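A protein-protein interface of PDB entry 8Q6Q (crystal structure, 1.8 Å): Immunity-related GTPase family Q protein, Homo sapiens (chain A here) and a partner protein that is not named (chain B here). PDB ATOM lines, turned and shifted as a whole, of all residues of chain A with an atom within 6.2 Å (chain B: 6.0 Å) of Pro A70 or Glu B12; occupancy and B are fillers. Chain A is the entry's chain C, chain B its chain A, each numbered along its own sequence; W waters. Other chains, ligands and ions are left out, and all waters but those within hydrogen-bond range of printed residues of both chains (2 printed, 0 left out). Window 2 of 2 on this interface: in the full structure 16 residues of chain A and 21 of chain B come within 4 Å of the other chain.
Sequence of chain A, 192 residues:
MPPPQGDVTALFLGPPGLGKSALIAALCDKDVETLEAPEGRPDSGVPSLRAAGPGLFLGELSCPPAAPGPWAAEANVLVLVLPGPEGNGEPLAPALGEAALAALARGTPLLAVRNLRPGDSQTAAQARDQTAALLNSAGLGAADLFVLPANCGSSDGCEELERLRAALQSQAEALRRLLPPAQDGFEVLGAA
Ala A67 touches none of the printed residues of chain B. Of the printed residues of chain B, Pro A70 touches Glu B12. Of the printed residues of chain B, Glu A74 touches Ser B10 (3.7 Å), Glu B12 (3.9 Å), His B13 (3.2 Å) and Val B16 (3.9 Å). Printed residues of chain A within 4 Å of Ser B10: Glu A74. Of chain A, only Pro A70, Trp A71 and Glu A74 come within 4 Å of Glu B12. Arg B14 touches none of the printed residues of chain A. Printed residues of chain A within 4 Å of Cys B15: Pro A47 and Trp A71. The nearest residue of chain B that does not touch Pro A70 is Ser B10 (5.0 Å). The nearest residue of chain A that does not touch Glu B12 is Ala A67 (5.4 Å). The nearest printed residue of chain A that does not touch Val B16 is Pro A47 (4.6 Å).
Water W1 lies within hydrogen-bond range of OG of Ser B10 (2.7 Å), O of Pro A70 (2.8 Å) and OE2 of Glu A74 (2.8 Å). Water W2 lies within hydrogen-bond range of the backbone carbonyl oxygen (O) of Ala A67 (2.8 Å), the indole nitrogen (NE1) of Trp A71 (3.2 Å) and the side-chain carboxylate (OE2) of Glu B12 (3.2 Å).
Among the printed residues, merely in contact across the chains: Pro A70 with Glu B12, Trp A71 with Glu B12, Trp A71 with Cys B15, Trp A71 with Val B16, Pro A47 with Cys B15, Glu A74 with Ser B10, Glu A74 with Val B16 and Glu A74 with Glu B12.
Printed residues of chain A that touch a printed residue of chain B: Pro A47, Pro A70, Trp A71 and Glu A74. Hydrophobic or aromatic side chains of chain A that line the printed part of chain B: Pro A47, Pro A70 and Trp A71. Hydrophobic or aromatic side chains of chain B that line the printed part of chain A: His B13 and Val B16.
OG of Ser B10 sits close to N of Glu B12 (3.5 Å). OG of Ser B10 lies within hydrogen-bond range of N of His B13 (2.9 Å). O of Leu B11 lies within hydrogen-bond range of SG of Cys B15. A ring nitrogen (NE2) of His B13 sits at hydrogen-bond distance from the side-chain carboxylate of Glu B17 (3.3 Å).
A ring nitrogen (ND1) of His B13 is in hydrogen-bond range of the side-chain carboxylate of Glu A74 (3.2 Å).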
ATOM      1  N   PRO A  47      23.001 -16.073  22.005  1.00  0.00           N
ATOM      2  CA  PRO A  47      23.831 -17.269  22.244  1.00  0.00           C
ATOM      3  C   PRO A  47      25.331 -16.954  22.283  1.00  0.00           C
ATOM      4  O   PRO A  47      25.861 -16.400  21.318  1.00  0.00           O
ATOM      5  CB  PRO A  47      23.538 -18.153  21.036  1.00  0.00           C
ATOM      6  CG  PRO A  47      23.364 -17.173  19.930  1.00  0.00           C
ATOM      7  CD  PRO A  47      22.783 -15.866  20.563  1.00  0.00           C
ATOM      8  N   ALA A  67      12.248 -22.832  20.998  1.00  0.00           N
ATOM      9  CA  ALA A  67      11.850 -23.877  20.036  1.00  0.00           C
ATOM     10  C   ALA A  67      13.123 -24.491  19.486  1.00  0.00           C
ATOM     11  O   ALA A  67      13.980 -23.754  18.955  1.00  0.00           O
ATOM     12  CB  ALA A  67      11.000 -23.316  18.904  1.00  0.00           C
ATOM     13  N   PRO A  68      13.326 -25.809  19.623  1.00  0.00           N
ATOM     14  CA  PRO A  68      14.617 -26.361  19.223  1.00  0.00           C
ATOM     15  C   PRO A  68      14.849 -26.367  17.717  1.00  0.00           C
ATOM     16  O   PRO A  68      16.015 -26.272  17.273  1.00  0.00           O
ATOM     17  CB  PRO A  68      14.585 -27.791  19.822  1.00  0.00           C
ATOM     18  CG  PRO A  68      13.066 -28.149  19.941  1.00  0.00           C
ATOM     19  CD  PRO A  68      12.434 -26.801  20.272  1.00  0.00           C
ATOM     20  N   GLY A  69      13.793 -26.526  16.920  1.00  0.00           N
ATOM     21  CA  GLY A  69      13.916 -26.711  15.495  1.00  0.00           C
ATOM     22  C   GLY A  69      14.778 -25.677  14.802  1.00  0.00           C
ATOM     23  O   GLY A  69      15.744 -25.998  14.105  1.00  0.00           O
ATOM     24  N   PRO A  70      14.434 -24.397  14.973  1.00  0.00           N
ATOM     25  CA  PRO A  70      15.180 -23.351  14.263  1.00  0.00           C
ATOM     26  C   PRO A  70      16.615 -23.207  14.724  1.00  0.00           C
ATOM     27  O   PRO A  70      17.472 -22.737  13.961  1.00  0.00           O
ATOM     28  CB  PRO A  70      14.370 -22.088  14.568  1.00  0.00           C
ATOM     29  CG  PRO A  70      12.970 -22.585  14.952  1.00  0.00           C
ATOM     30  CD  PRO A  70      13.254 -23.871  15.682  1.00  0.00           C
ATOM     31  N   TRP A  71      16.906 -23.592  15.952  1.00  0.00           N
ATOM     32  CA  TRP A  71      18.291 -23.544  16.422  1.00  0.00           C
ATOM     33  C   TRP A  71      19.064 -24.732  15.892  1.00  0.00           C
ATOM     34  O   TRP A  71      20.186 -24.602  15.383  1.00  0.00           O
ATOM     35  CB  TRP A  71      18.311 -23.555  17.944  1.00  0.00           C
ATOM     36  CG  TRP A  71      17.982 -22.255  18.551  1.00  0.00           C
ATOM     37  CD1 TRP A  71      16.864 -21.925  19.251  1.00  0.00           C
ATOM     38  CD2 TRP A  71      18.801 -21.064  18.490  1.00  0.00           C
ATOM     39  NE1 TRP A  71      16.958 -20.576  19.670  1.00  0.00           N
ATOM     40  CE2 TRP A  71      18.134 -20.055  19.198  1.00  0.00           C
ATOM     41  CE3 TRP A  71      20.044 -20.784  17.915  1.00  0.00           C
ATOM     42  CZ2 TRP A  71      18.649 -18.747  19.309  1.00  0.00           C
ATOM     43  CZ3 TRP A  71      20.572 -19.479  18.044  1.00  0.00           C
ATOM     44  CH2 TRP A  71      19.878 -18.506  18.746  1.00  0.00           C
ATOM     45  N   ALA A  72      18.466 -25.908  16.010  1.00  0.00           N
ATOM     46  CA  ALA A  72      19.125 -27.114  15.519  1.00  0.00           C
ATOM     47  C   ALA A  72      19.424 -27.018  14.029  1.00  0.00           C
ATOM     48  O   ALA A  72      20.415 -27.584  13.549  1.00  0.00           O
ATOM     49  CB  ALA A  72      18.226 -28.328  15.849  1.00  0.00           C
ATOM     50  N   ALA A  73      18.599 -26.289  13.284  1.00  0.00           N
ATOM     51  CA  ALA A  73      18.836 -26.074  11.866  1.00  0.00           C
ATOM     52  C   ALA A  73      20.158 -25.358  11.612  1.00  0.00           C
ATOM     53  O   ALA A  73      20.696 -25.447  10.500  1.00  0.00           O
ATOM     54  CB  ALA A  73      17.691 -25.236  11.277  1.00  0.00           C
ATOM     55  N   GLU A  74      20.676 -24.632  12.607  1.00  0.00           N
ATOM     56  CA  GLU A  74      21.947 -23.906  12.516  1.00  0.00           C
ATOM     57  C   GLU A  74      23.108 -24.700  13.080  1.00  0.00           C
ATOM     58  O   GLU A  74      24.251 -24.260  12.961  1.00  0.00           O
ATOM     59  CB  GLU A  74      21.856 -22.568  13.288  1.00  0.00           C
ATOM     60  CG  GLU A  74      20.729 -21.648  12.833  1.00  0.00           C
ATOM     61  CD  GLU A  74      20.703 -21.434  11.352  1.00  0.00           C
ATOM     62  OE1 GLU A  74      21.787 -21.279  10.751  1.00  0.00           O
ATOM     63  OE2 GLU A  74      19.585 -21.384  10.781  1.00  0.00           O
ATOM     64  N   SER B  10      16.666 -16.383   9.124  1.00  0.00           N
ATOM     65  CA  SER B  10      16.002 -16.548  10.400  1.00  0.00           C
ATOM     66  C   SER B  10      16.749 -15.820  11.507  1.00  0.00           C
ATOM     67  O   SER B  10      17.964 -15.583  11.442  1.00  0.00           O
ATOM     68  CB  SER B  10      15.859 -18.045  10.743  1.00  0.00           C
ATOM     69  OG  SER B  10      17.097 -18.610  11.172  1.00  0.00           O
ATOM     70  N   LEU B  11      15.995 -15.483  12.552  1.00  0.00           N
ATOM     71  CA  LEU B  11      16.593 -14.911  13.744  1.00  0.00           C
ATOM     72  C   LEU B  11      17.711 -15.800  14.248  1.00  0.00           C
ATOM     73  O   LEU B  11      18.784 -15.308  14.621  1.00  0.00           O
ATOM     74  CB  LEU B  11      15.531 -14.717  14.833  1.00  0.00           C
ATOM     75  CG  LEU B  11      16.041 -14.258  16.206  1.00  0.00           C
ATOM     76  CD1 LEU B  11      16.882 -12.946  16.089  1.00  0.00           C
ATOM     77  CD2 LEU B  11      14.953 -14.089  17.273  1.00  0.00           C
ATOM     78  N   GLU B  12      17.466 -17.128  14.284  1.00  0.00           N
ATOM     79  CA  GLU B  12      18.495 -18.028  14.784  1.00  0.00           C
ATOM     80  C   GLU B  12      19.722 -18.001  13.894  1.00  0.00           C
ATOM     81  O   GLU B  12      20.849 -17.973  14.388  1.00  0.00           O
ATOM     82  CB  GLU B  12      17.960 -19.456  14.934  1.00  0.00           C
ATOM     83  CG  GLU B  12      16.859 -19.547  16.002  1.00  0.00           C
ATOM     84  CD  GLU B  12      15.489 -19.031  15.513  1.00  0.00           C
ATOM     85  OE1 GLU B  12      15.340 -18.639  14.322  1.00  0.00           O
ATOM     86  OE2 GLU B  12      14.534 -19.089  16.318  1.00  0.00           O
ATOM     87  N   HIS B  13      19.529 -18.030  12.586  1.00  0.00           N
ATOM     88  CA  HIS B  13      20.669 -17.930  11.689  1.00  0.00           C
ATOM     89  C   HIS B  13      21.478 -16.673  11.992  1.00  0.00           C
ATOM     90  O   HIS B  13      22.714 -16.722  12.063  1.00  0.00           O
ATOM     91  CB  HIS B  13      20.171 -17.918  10.252  1.00  0.00           C
ATOM     92  CG  HIS B  13      21.264 -17.857   9.228  1.00  0.00           C
ATOM     93  ND1 HIS B  13      21.646 -18.959   8.502  1.00  0.00           N
ATOM     94  CD2 HIS B  13      22.034 -16.831   8.788  1.00  0.00           C
ATOM     95  CE1 HIS B  13      22.619 -18.624   7.672  1.00  0.00           C
ATOM     96  NE2 HIS B  13      22.861 -17.338   7.808  1.00  0.00           N
ATOM     97  N   ARG B  14      20.791 -15.543  12.195  1.00  0.00           N
ATOM     98  CA  ARG B  14      21.513 -14.289  12.414  1.00  0.00           C
ATOM     99  C   ARG B  14      22.262 -14.321  13.747  1.00  0.00           C
ATOM    100  O   ARG B  14      23.440 -13.932  13.820  1.00  0.00           O
ATOM    101  CB  ARG B  14      20.525 -13.122  12.311  1.00  0.00           C
ATOM    102  CG  ARG B  14      20.120 -12.903  10.843  1.00  0.00           C
ATOM    103  CD  ARG B  14      19.159 -11.705  10.645  1.00  0.00           C
ATOM    104  NE  ARG B  14      17.764 -12.098  10.839  1.00  0.00           N
ATOM    105  CZ  ARG B  14      16.988 -11.698  11.846  1.00  0.00           C
ATOM    106  NH1 ARG B  14      17.439 -10.898  12.794  1.00  0.00           N
ATOM    107  NH2 ARG B  14      15.723 -12.106  11.899  1.00  0.00           N
ATOM    108  N   CYS B  15      21.621 -14.845  14.800  1.00  0.00           N
ATOM    109  CA  CYS B  15      22.298 -14.984  16.094  1.00  0.00           C
ATOM    110  C   CYS B  15      23.595 -15.790  15.998  1.00  0.00           C
ATOM    111  O   CYS B  15      24.633 -15.369  16.526  1.00  0.00           O
ATOM    112  CB  CYS B  15      21.365 -15.623  17.110  1.00  0.00           C
ATOM    113  SG  CYS B  15      20.081 -14.550  17.642  1.00  0.00           S
ATOM    114  N   VAL B  16      23.546 -16.980  15.376  1.00  0.00           N
ATOM    115  CA  VAL B  16      24.744 -17.812  15.303  1.00  0.00           C
ATOM    116  C   VAL B  16      25.808 -17.107  14.466  1.00  0.00           C
ATOM    117  O   VAL B  16      27.003 -17.132  14.800  1.00  0.00           O
ATOM    118  CB  VAL B  16      24.410 -19.212  14.745  1.00  0.00           C
ATOM    119  CG1 VAL B  16      25.660 -19.984  14.399  1.00  0.00           C
ATOM    120  CG2 VAL B  16      23.448 -20.002  15.730  1.00  0.00           C
ATOM    121  N   GLU B  17      25.383 -16.432  13.392  1.00  0.00           N
ATOM    122  CA  GLU B  17      26.322 -15.706  12.540  1.00  0.00           C
ATOM    123  C   GLU B  17      27.083 -14.647  13.318  1.00  0.00           C
ATOM    124  O   GLU B  17      28.319 -14.577  13.245  1.00  0.00           O
ATOM    125  CB  GLU B  17      25.595 -15.082  11.355  1.00  0.00           C
ATOM    126  CG  GLU B  17      26.530 -14.666  10.253  1.00  0.00           C
ATOM    127  CD  GLU B  17      25.807 -14.213   9.000  1.00  0.00           C
ATOM    128  OE1 GLU B  17      24.752 -14.804   8.641  1.00  0.00           O
ATOM    129  OE2 GLU B  17      26.284 -13.238   8.398  1.00  0.00           O
HETATM  130  O   HOH W   1      16.918 -21.214  11.729  1.00  0.00           O
HETATM  131  O   HOH W   2      13.911 -20.989  18.809  1.00  0.00           O
